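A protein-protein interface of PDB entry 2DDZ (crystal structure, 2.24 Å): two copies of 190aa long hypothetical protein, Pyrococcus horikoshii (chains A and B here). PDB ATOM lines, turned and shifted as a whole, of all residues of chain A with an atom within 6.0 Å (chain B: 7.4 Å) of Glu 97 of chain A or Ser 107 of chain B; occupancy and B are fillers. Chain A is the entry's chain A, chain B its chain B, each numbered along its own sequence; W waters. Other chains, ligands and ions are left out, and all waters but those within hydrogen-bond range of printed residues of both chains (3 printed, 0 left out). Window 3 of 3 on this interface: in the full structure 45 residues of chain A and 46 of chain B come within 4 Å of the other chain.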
ATOM      1  N   ILE A  92       4.202  13.154   9.113  1.00  0.00           N
ATOM      2  CA  ILE A  92       2.963  12.889   8.379  1.00  0.00           C
ATOM      3  C   ILE A  92       1.839  13.736   8.973  1.00  0.00           C
ATOM      4  O   ILE A  92       1.053  14.349   8.245  1.00  0.00           O
ATOM      5  CB  ILE A  92       2.610  11.388   8.444  1.00  0.00           C
ATOM      6  CG1 ILE A  92       3.679  10.584   7.696  1.00  0.00           C
ATOM      7  CG2 ILE A  92       1.234  11.141   7.861  1.00  0.00           C
ATOM      8  CD1 ILE A  92       3.781  10.946   6.230  1.00  0.00           C
ATOM      9  N   ALA A  93       1.776  13.789  10.302  1.00  0.00           N
ATOM     10  CA  ALA A  93       0.756  14.584  10.967  1.00  0.00           C
ATOM     11  C   ALA A  93       0.876  16.076  10.607  1.00  0.00           C
ATOM     12  O   ALA A  93      -0.137  16.764  10.471  1.00  0.00           O
ATOM     13  CB  ALA A  93       0.845  14.382  12.471  1.00  0.00           C
ATOM     14  N   ARG A  94       2.102  16.575  10.434  1.00  0.00           N
ATOM     15  CA  ARG A  94       2.293  17.979  10.064  1.00  0.00           C
ATOM     16  C   ARG A  94       1.744  18.244   8.658  1.00  0.00           C
ATOM     17  O   ARG A  94       1.115  19.269   8.420  1.00  0.00           O
ATOM     18  CB  ARG A  94       3.772  18.373  10.089  1.00  0.00           C
ATOM     19  CG  ARG A  94       4.008  19.833   9.684  1.00  0.00           C
ATOM     20  CD  ARG A  94       3.556  20.780  10.801  1.00  0.00           C
ATOM     21  NE  ARG A  94       3.630  22.193  10.442  1.00  0.00           N
ATOM     22  CZ  ARG A  94       2.665  22.860   9.812  1.00  0.00           C
ATOM     23  NH1 ARG A  94       1.547  22.242   9.460  1.00  0.00           N
ATOM     24  NH2 ARG A  94       2.810  24.150   9.543  1.00  0.00           N
ATOM     25  N   LEU A  95       2.006  17.327   7.730  1.00  0.00           N
ATOM     26  CA  LEU A  95       1.510  17.461   6.358  1.00  0.00           C
ATOM     27  C   LEU A  95      -0.013  17.445   6.339  1.00  0.00           C
ATOM     28  O   LEU A  95      -0.636  18.173   5.567  1.00  0.00           O
ATOM     29  CB  LEU A  95       2.027  16.328   5.476  1.00  0.00           C
ATOM     30  CG  LEU A  95       3.542  16.222   5.386  1.00  0.00           C
ATOM     31  CD1 LEU A  95       3.943  14.965   4.634  1.00  0.00           C
ATOM     32  CD2 LEU A  95       4.086  17.464   4.710  1.00  0.00           C
ATOM     33  N   VAL A  96      -0.619  16.624   7.192  1.00  0.00           N
ATOM     34  CA  VAL A  96      -2.075  16.576   7.217  1.00  0.00           C
ATOM     35  C   VAL A  96      -2.636  17.912   7.704  1.00  0.00           C
ATOM     36  O   VAL A  96      -3.666  18.362   7.212  1.00  0.00           O
ATOM     37  CB  VAL A  96      -2.615  15.417   8.106  1.00  0.00           C
ATOM     38  CG1 VAL A  96      -4.142  15.474   8.180  1.00  0.00           C
ATOM     39  CG2 VAL A  96      -2.209  14.082   7.508  1.00  0.00           C
ATOM     40  N   GLU A  97      -1.957  18.560   8.650  1.00  0.00           N
ATOM     41  CA  GLU A  97      -2.451  19.847   9.138  1.00  0.00           C
ATOM     42  C   GLU A  97      -2.234  20.901   8.060  1.00  0.00           C
ATOM     43  O   GLU A  97      -3.072  21.768   7.841  1.00  0.00           O
ATOM     44  CB  GLU A  97      -1.749  20.269  10.433  1.00  0.00           C
ATOM     45  CG  GLU A  97      -2.501  21.390  11.141  1.00  0.00           C
ATOM     46  CD  GLU A  97      -1.957  21.720  12.518  1.00  0.00           C
ATOM     47  OE1 GLU A  97      -1.060  20.992  12.980  1.00  0.00           O
ATOM     48  OE2 GLU A  97      -2.432  22.704  13.138  1.00  0.00           O
ATOM     49  N   LEU A  98      -1.100  20.808   7.378  1.00  0.00           N
ATOM     50  CA  LEU A  98      -0.782  21.738   6.313  1.00  0.00           C
ATOM     51  C   LEU A  98      -1.833  21.699   5.199  1.00  0.00           C
ATOM     52  O   LEU A  98      -2.242  22.737   4.682  1.00  0.00           O
ATOM     53  CB  LEU A  98       0.600  21.410   5.746  1.00  0.00           C
ATOM     54  CG  LEU A  98       1.030  22.251   4.540  1.00  0.00           C
ATOM     55  CD1 LEU A  98       0.932  23.730   4.890  1.00  0.00           C
ATOM     56  CD2 LEU A  98       2.448  21.880   4.135  1.00  0.00           C
ATOM     57  N   LEU A  99      -2.286  20.503   4.837  1.00  0.00           N
ATOM     58  CA  LEU A  99      -3.283  20.372   3.784  1.00  0.00           C
ATOM     59  C   LEU A  99      -4.578  21.133   4.084  1.00  0.00           C
ATOM     60  O   LEU A  99      -5.247  21.615   3.166  1.00  0.00           O
ATOM     61  CB  LEU A  99      -3.564  18.885   3.524  1.00  0.00           C
ATOM     62  CG  LEU A  99      -2.400  18.216   2.780  1.00  0.00           C
ATOM     63  CD1 LEU A  99      -2.505  16.704   2.804  1.00  0.00           C
ATOM     64  CD2 LEU A  99      -2.396  18.717   1.357  1.00  0.00           C
ATOM     65  N   TRP A 100      -4.927  21.257   5.363  1.00  0.00           N
ATOM     66  CA  TRP A 100      -6.144  21.968   5.739  1.00  0.00           C
ATOM     67  C   TRP A 100      -5.995  23.459   5.410  1.00  0.00           C
ATOM     68  O   TRP A 100      -6.987  24.157   5.190  1.00  0.00           O
ATOM     69  CB  TRP A 100      -6.449  21.769   7.240  1.00  0.00           C
ATOM     70  CG  TRP A 100      -7.689  22.512   7.729  1.00  0.00           C
ATOM     71  CD1 TRP A 100      -7.775  23.323   8.833  1.00  0.00           C
ATOM     72  CD2 TRP A 100      -8.998  22.519   7.130  1.00  0.00           C
ATOM     73  NE1 TRP A 100      -9.048  23.833   8.953  1.00  0.00           N
ATOM     74  CE2 TRP A 100      -9.819  23.357   7.925  1.00  0.00           C
ATOM     75  CE3 TRP A 100      -9.556  21.903   5.999  1.00  0.00           C
ATOM     76  CZ2 TRP A 100     -11.167  23.593   7.626  1.00  0.00           C
ATOM     77  CZ3 TRP A 100     -10.898  22.136   5.703  1.00  0.00           C
ATOM     78  CH2 TRP A 100     -11.689  22.977   6.519  1.00  0.00           C
ATOM     79  N   ASN A 101      -4.755  23.948   5.375  1.00  0.00           N
ATOM     80  CA  ASN A 101      -4.516  25.350   5.055  1.00  0.00           C
ATOM     81  C   ASN A 101      -4.823  25.602   3.577  1.00  0.00           C
ATOM     82  O   ASN A 101      -4.894  26.743   3.126  1.00  0.00           O
ATOM     83  CB  ASN A 101      -3.065  25.745   5.364  1.00  0.00           C
ATOM     84  CG  ASN A 101      -2.860  27.248   5.316  1.00  0.00           C
ATOM     85  OD1 ASN A 101      -2.102  27.763   4.492  1.00  0.00           O
ATOM     86  ND2 ASN A 101      -3.555  27.965   6.197  1.00  0.00           N
ATOM     87  N   ILE B  92       0.595  15.352  21.052  1.00  0.00           N
ATOM     88  CA  ILE B  92      -0.135  16.618  21.024  1.00  0.00           C
ATOM     89  C   ILE B  92      -0.873  16.703  19.686  1.00  0.00           C
ATOM     90  O   ILE B  92      -2.024  17.123  19.628  1.00  0.00           O
ATOM     91  CB  ILE B  92       0.825  17.823  21.124  1.00  0.00           C
ATOM     92  CG1 ILE B  92       1.457  17.849  22.516  1.00  0.00           C
ATOM     93  CG2 ILE B  92       0.075  19.145  20.908  1.00  0.00           C
ATOM     94  CD1 ILE B  92       0.452  18.047  23.629  1.00  0.00           C
ATOM     95  N   ALA B  93      -0.201  16.284  18.614  1.00  0.00           N
ATOM     96  CA  ALA B  93      -0.788  16.317  17.280  1.00  0.00           C
ATOM     97  C   ALA B  93      -1.988  15.377  17.179  1.00  0.00           C
ATOM     98  O   ALA B  93      -2.969  15.693  16.512  1.00  0.00           O
ATOM     99  CB  ALA B  93       0.269  15.944  16.230  1.00  0.00           C
ATOM    100  N   VAL B  96      -4.928  17.061  18.664  1.00  0.00           N
ATOM    101  CA  VAL B  96      -5.463  18.091  17.779  1.00  0.00           C
ATOM    102  C   VAL B  96      -6.372  17.450  16.732  1.00  0.00           C
ATOM    103  O   VAL B  96      -7.446  17.963  16.421  1.00  0.00           O
ATOM    104  CB  VAL B  96      -4.335  18.853  17.031  1.00  0.00           C
ATOM    105  CG1 VAL B  96      -4.933  19.815  15.998  1.00  0.00           C
ATOM    106  CG2 VAL B  96      -3.501  19.626  18.014  1.00  0.00           C
ATOM    107  N   GLU B  97      -5.928  16.330  16.178  1.00  0.00           N
ATOM    108  CA  GLU B  97      -6.708  15.629  15.160  1.00  0.00           C
ATOM    109  C   GLU B  97      -8.004  15.126  15.782  1.00  0.00           C
ATOM    110  O   GLU B  97      -9.034  15.033  15.120  1.00  0.00           O
ATOM    111  CB  GLU B  97      -5.908  14.446  14.598  1.00  0.00           C
ATOM    112  CG  GLU B  97      -4.674  14.838  13.777  1.00  0.00           C
ATOM    113  CD  GLU B  97      -3.734  13.657  13.524  1.00  0.00           C
ATOM    114  OE1 GLU B  97      -3.791  12.682  14.302  1.00  0.00           O
ATOM    115  OE2 GLU B  97      -2.925  13.710  12.567  1.00  0.00           O
ATOM    116  N   LEU B  99      -9.620  16.587  18.342  1.00  0.00           N
ATOM    117  CA  LEU B  99     -10.477  17.741  18.539  1.00  0.00           C
ATOM    118  C   LEU B  99     -11.305  18.041  17.280  1.00  0.00           C
ATOM    119  O   LEU B  99     -12.458  18.459  17.385  1.00  0.00           O
ATOM    120  CB  LEU B  99      -9.629  18.955  18.966  1.00  0.00           C
ATOM    121  CG  LEU B  99      -9.108  18.919  20.417  1.00  0.00           C
ATOM    122  CD1 LEU B  99      -8.126  20.057  20.689  1.00  0.00           C
ATOM    123  CD2 LEU B  99     -10.292  19.022  21.365  1.00  0.00           C
ATOM    124  N   TRP B 100     -10.728  17.825  16.095  1.00  0.00           N
ATOM    125  CA  TRP B 100     -11.464  18.071  14.859  1.00  0.00           C
ATOM    126  C   TRP B 100     -12.728  17.206  14.846  1.00  0.00           C
ATOM    127  O   TRP B 100     -13.769  17.630  14.355  1.00  0.00           O
ATOM    128  CB  TRP B 100     -10.613  17.762  13.607  1.00  0.00           C
ATOM    129  CG  TRP B 100      -9.324  18.551  13.484  1.00  0.00           C
ATOM    130  CD1 TRP B 100      -9.056  19.781  14.019  1.00  0.00           C
ATOM    131  CD2 TRP B 100      -8.131  18.155  12.780  1.00  0.00           C
ATOM    132  NE1 TRP B 100      -7.773  20.168  13.700  1.00  0.00           N
ATOM    133  CE2 TRP B 100      -7.185  19.189  12.942  1.00  0.00           C
ATOM    134  CE3 TRP B 100      -7.772  17.021  12.030  1.00  0.00           C
ATOM    135  CZ2 TRP B 100      -5.902  19.129  12.383  1.00  0.00           C
ATOM    136  CZ3 TRP B 100      -6.495  16.959  11.474  1.00  0.00           C
ATOM    137  CH2 TRP B 100      -5.575  18.009  11.656  1.00  0.00           C
ATOM    138  N   ILE B 104     -14.044  21.030  16.551  1.00  0.00           N
ATOM    139  CA  ILE B 104     -13.211  22.111  17.062  1.00  0.00           C
ATOM    140  C   ILE B 104     -12.142  22.483  16.056  1.00  0.00           C
ATOM    141  O   ILE B 104     -11.516  21.610  15.453  1.00  0.00           O
ATOM    142  CB  ILE B 104     -12.477  21.701  18.343  1.00  0.00           C
ATOM    143  CG1 ILE B 104     -13.479  21.172  19.379  1.00  0.00           C
ATOM    144  CG2 ILE B 104     -11.688  22.901  18.880  1.00  0.00           C
ATOM    145  CD1 ILE B 104     -14.511  22.189  19.835  1.00  0.00           C
ATOM    146  N   GLU B 105     -11.921  23.778  15.881  1.00  0.00           N
ATOM    147  CA  GLU B 105     -10.901  24.241  14.952  1.00  0.00           C
ATOM    148  C   GLU B 105      -9.622  24.382  15.770  1.00  0.00           C
ATOM    149  O   GLU B 105      -9.246  25.474  16.189  1.00  0.00           O
ATOM    150  CB  GLU B 105     -11.294  25.591  14.340  1.00  0.00           C
ATOM    151  CG  GLU B 105     -10.291  26.121  13.310  1.00  0.00           C
ATOM    152  CD  GLU B 105     -10.351  25.387  11.977  1.00  0.00           C
ATOM    153  OE1 GLU B 105     -11.210  25.739  11.139  1.00  0.00           O
ATOM    154  OE2 GLU B 105      -9.546  24.454  11.771  1.00  0.00           O
ATOM    155  N   ALA B 106      -8.971  23.254  16.008  1.00  0.00           N
ATOM    156  CA  ALA B 106      -7.742  23.232  16.784  1.00  0.00           C
ATOM    157  C   ALA B 106      -6.510  23.198  15.885  1.00  0.00           C
ATOM    158  O   ALA B 106      -6.492  22.530  14.842  1.00  0.00           O
ATOM    159  CB  ALA B 106      -7.744  22.019  17.707  1.00  0.00           C
ATOM    160  N   SER B 107      -5.479  23.922  16.298  1.00  0.00           N
ATOM    161  CA  SER B 107      -4.240  23.958  15.546  1.00  0.00           C
ATOM    162  C   SER B 107      -3.123  23.696  16.534  1.00  0.00           C
ATOM    163  O   SER B 107      -3.301  23.886  17.739  1.00  0.00           O
ATOM    164  CB  SER B 107      -4.040  25.326  14.886  1.00  0.00           C
ATOM    165  OG  SER B 107      -4.055  26.362  15.850  1.00  0.00           O
ATOM    166  N   ARG B 108      -1.981  23.250  16.020  1.00  0.00           N
ATOM    167  CA  ARG B 108      -0.825  22.975  16.853  1.00  0.00           C
ATOM    168  C   ARG B 108       0.290  23.990  16.614  1.00  0.00           C
ATOM    169  O   ARG B 108       0.458  24.487  15.499  1.00  0.00           O
ATOM    170  CB  ARG B 108      -0.289  21.568  16.571  1.00  0.00           C
ATOM    171  CG  ARG B 108       0.945  21.213  17.401  1.00  0.00           C
ATOM    172  CD  ARG B 108       1.288  19.743  17.300  1.00  0.00           C
ATOM    173  NE  ARG B 108       1.630  19.339  15.938  1.00  0.00           N
ATOM    174  CZ  ARG B 108       2.858  19.366  15.427  1.00  0.00           C
ATOM    175  NH1 ARG B 108       3.885  19.782  16.166  1.00  0.00           N
ATOM    176  NH2 ARG B 108       3.063  18.975  14.175  1.00  0.00           N
ATOM    177  N   ARG B 109       1.030  24.299  17.676  1.00  0.00           N
ATOM    178  CA  ARG B 109       2.182  25.206  17.615  1.00  0.00           C
ATOM    179  C   ARG B 109       3.237  24.536  18.479  1.00  0.00           C
ATOM    180  O   ARG B 109       3.345  24.813  19.676  1.00  0.00           O
ATOM    181  CB  ARG B 109       1.849  26.587  18.177  1.00  0.00           C
ATOM    182  CG  ARG B 109       0.763  27.320  17.417  1.00  0.00           C
ATOM    183  CD  ARG B 109       0.600  28.735  17.926  1.00  0.00           C
ATOM    184  NE  ARG B 109      -0.644  29.328  17.441  1.00  0.00           N
ATOM    185  CZ  ARG B 109      -1.081  30.530  17.790  1.00  0.00           C
ATOM    186  NH1 ARG B 109      -0.364  31.270  18.629  1.00  0.00           N
ATOM    187  NH2 ARG B 109      -2.234  30.983  17.309  1.00  0.00           N
ATOM    188  N   GLY B 110       3.990  23.628  17.867  1.00  0.00           N
ATOM    189  CA  GLY B 110       5.008  22.883  18.584  1.00  0.00           C
ATOM    190  C   GLY B 110       4.341  21.863  19.491  1.00  0.00           C
ATOM    191  O   GLY B 110       3.786  20.854  19.033  1.00  0.00           O
ATOM    192  N   ASP B 112       2.074  22.966  21.844  1.00  0.00           N
ATOM    193  CA  ASP B 112       0.865  23.594  22.365  1.00  0.00           C
ATOM    194  C   ASP B 112      -0.351  23.540  21.436  1.00  0.00           C
ATOM    195  O   ASP B 112      -0.243  23.691  20.210  1.00  0.00           O
ATOM    196  CB  ASP B 112       1.139  25.054  22.713  1.00  0.00           C
ATOM    197  CG  ASP B 112       2.170  25.213  23.810  1.00  0.00           C
ATOM    198  OD1 ASP B 112       2.245  24.329  24.688  1.00  0.00           O
ATOM    199  OD2 ASP B 112       2.896  26.234  23.806  1.00  0.00           O
ATOM    200  N   ILE B 113      -1.513  23.315  22.034  1.00  0.00           N
ATOM    201  CA  ILE B 113      -2.754  23.296  21.276  1.00  0.00           C
ATOM    202  C   ILE B 113      -3.446  24.646  21.414  1.00  0.00           C
ATOM    203  O   ILE B 113      -3.593  25.163  22.529  1.00  0.00           O
ATOM    204  CB  ILE B 113      -3.738  22.225  21.792  1.00  0.00           C
ATOM    205  CG1 ILE B 113      -3.129  20.839  21.638  1.00  0.00           C
ATOM    206  CG2 ILE B 113      -5.055  22.317  21.047  1.00  0.00           C
ATOM    207  CD1 ILE B 113      -2.312  20.743  20.399  1.00  0.00           C
ATOM    208  N   TYR B 114      -3.864  25.212  20.283  1.00  0.00           N
ATOM    209  CA  TYR B 114      -4.578  26.492  20.285  1.00  0.00           C
ATOM    210  C   TYR B 114      -5.938  26.385  19.613  1.00  0.00           C
ATOM    211  O   TYR B 114      -6.162  25.527  18.748  1.00  0.00           O
ATOM    212  CB  TYR B 114      -3.794  27.598  19.552  1.00  0.00           C
ATOM    213  CG  TYR B 114      -2.640  28.208  20.319  1.00  0.00           C
ATOM    214  CD1 TYR B 114      -1.445  27.516  20.482  1.00  0.00           C
ATOM    215  CD2 TYR B 114      -2.749  29.478  20.892  1.00  0.00           C
ATOM    216  CE1 TYR B 114      -0.379  28.065  21.199  1.00  0.00           C
ATOM    217  CE2 TYR B 114      -1.691  30.037  21.617  1.00  0.00           C
ATOM    218  CZ  TYR B 114      -0.508  29.321  21.765  1.00  0.00           C
ATOM    219  OH  TYR B 114       0.534  29.855  22.495  1.00  0.00           O
ATOM    220  N   VAL B 115      -6.843  27.265  20.031  1.00  0.00           N
ATOM    221  CA  VAL B 115      -8.184  27.376  19.453  1.00  0.00           C
ATOM    222  C   VAL B 115      -8.558  28.850  19.615  1.00  0.00           C
ATOM    223  O   VAL B 115      -8.460  29.403  20.714  1.00  0.00           O
ATOM    224  CB  VAL B 115      -9.222  26.484  20.172  1.00  0.00           C
ATOM    225  CG1 VAL B 115     -10.600  26.683  19.554  1.00  0.00           C
ATOM    226  CG2 VAL B 115      -8.823  25.028  20.054  1.00  0.00           C
ATOM    227  N   ASN B 116      -8.947  29.493  18.515  1.00  0.00           N
ATOM    228  CA  ASN B 116      -9.311  30.910  18.546  1.00  0.00           C
ATOM    229  C   ASN B 116      -8.136  31.756  19.027  1.00  0.00           C
ATOM    230  O   ASN B 116      -8.331  32.787  19.664  1.00  0.00           O
ATOM    231  CB  ASN B 116     -10.518  31.161  19.472  1.00  0.00           C
ATOM    232  CG  ASN B 116     -11.804  30.550  18.944  1.00  0.00           C
ATOM    233  OD1 ASN B 116     -12.064  30.575  17.742  1.00  0.00           O
ATOM    234  ND2 ASN B 116     -12.622  30.013  19.845  1.00  0.00           N
ATOM    235  N   GLY B 117      -6.920  31.312  18.741  1.00  0.00           N
ATOM    236  CA  GLY B 117      -5.756  32.070  19.155  1.00  0.00           C
ATOM    237  C   GLY B 117      -5.469  32.006  20.638  1.00  0.00           C
ATOM    238  O   GLY B 117      -4.637  32.765  21.143  1.00  0.00           O
ATOM    239  N   ARG B 118      -6.156  31.110  21.340  1.00  0.00           N
ATOM    240  CA  ARG B 118      -5.943  30.934  22.774  1.00  0.00           C
ATOM    241  C   ARG B 118      -5.363  29.553  23.068  1.00  0.00           C
ATOM    242  O   ARG B 118      -5.748  28.567  22.435  1.00  0.00           O
ATOM    243  CB  ARG B 118      -7.261  31.125  23.522  1.00  0.00           C
ATOM    244  CG  ARG B 118      -7.749  32.556  23.469  1.00  0.00           C
ATOM    245  CD  ARG B 118      -9.252  32.630  23.366  1.00  0.00           C
ATOM    246  NE  ARG B 118      -9.915  32.309  24.624  1.00  0.00           N
ATOM    247  CZ  ARG B 118     -11.215  32.058  24.726  1.00  0.00           C
ATOM    248  NH1 ARG B 118     -11.982  32.091  23.639  1.00  0.00           N
ATOM    249  NH2 ARG B 118     -11.747  31.773  25.906  1.00  0.00           N
HETATM  250  O   HOH W   1       0.076  18.864  13.336  1.00  0.00           O
HETATM  251  O   HOH W   2       1.288  22.665  13.348  1.00  0.00           O
HETATM  252  O   HOH W   3      -2.536  16.259  11.756  1.00  0.00           O
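Water W1 lies within hydrogen-bond range of the side-chain carboxylate of Glu 97 of chain A and the guanidinium group of Arg 108 of chain B. Water W3 lies within hydrogen-bond range of the side-chain carboxylate (OE2) of Glu 97 of chain B (2.7 Å) and the backbone carbonyl oxygen (O) of Ala 93 of chain A (2.8 Å). Water W2 lies within hydrogen-bond range of the side-chain carboxylate of Glu 97 of chain A and the backbone carbonyl oxygen of Arg 108 of chain B.
Of the printed residues of chain B, Ala 93 of chain A touches Glu 97 (3.8 Å). Of chain B, only Ser 107 and Arg 108 come within 4 Å of Glu 97 of chain A. Ala 93 of chain B touches none of the printed residues of chain A. Of chain A, only Glu 97 (3.3 Å) comes within 4 Å of Ser 107 of chain B. Of the printed residues of chain A, Arg 108 of chain B touches Arg 94 and Glu 97. Gly 110 of chain B touches none of the printed residues of chain A. The nearest residue of chain B that does not touch Glu 97 of chain A is Trp 100 of chain B (4.3 Å). The nearest printed residue of chain A that does not touch Glu 105 of chain B is Glu 97 of chain A (7.5 Å).
Of the 10 printed residues of chain A, 4 touch a printed residue of chain B. Hydrophobic or aromatic side chains of chain A that line the printed part of chain B: Ala 93 and Trp 100.
O of Ser 107 of chain B is in hydrogen-bond range of N of Tyr 114 of chain B (2.9 Å). The guanidinium group of Arg 108 of chain B is in hydrogen-bond range of the backbone carbonyl oxygen of Gly 110 of chain B (3.1 Å).
Glu 97 of chain B touches Ala 93 of chain A. Arg 108 of chain B touches Arg 94 of chain A (NH2 to CD, 3.9 Å). Glu 97 of chain A touches Ser 107 of chain B (OE2 to CA, 3.3 Å).
Ala 93 of chain A touches Glu 97 of chain B, but with the chains exchanged Glu 97 of chain A does not touch Ala 93 of chain B (6.1 Å). Of the 5 pairs that touch across the chains among the printed residues, none has its exchanged pair printed and touching as well.
The side-chain carboxylate (OE2) of Glu 97 of chain A is in hydrogen-bond range of the backbone NH (N) of Arg 108 of chain B, at 3.0 Å. The indole nitrogen (NE1) of Trp 100 of chain A sits at hydrogen-bond distance from the side-chain carboxylate (OE2) of Glu 105 of chain B (2.9 Å).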
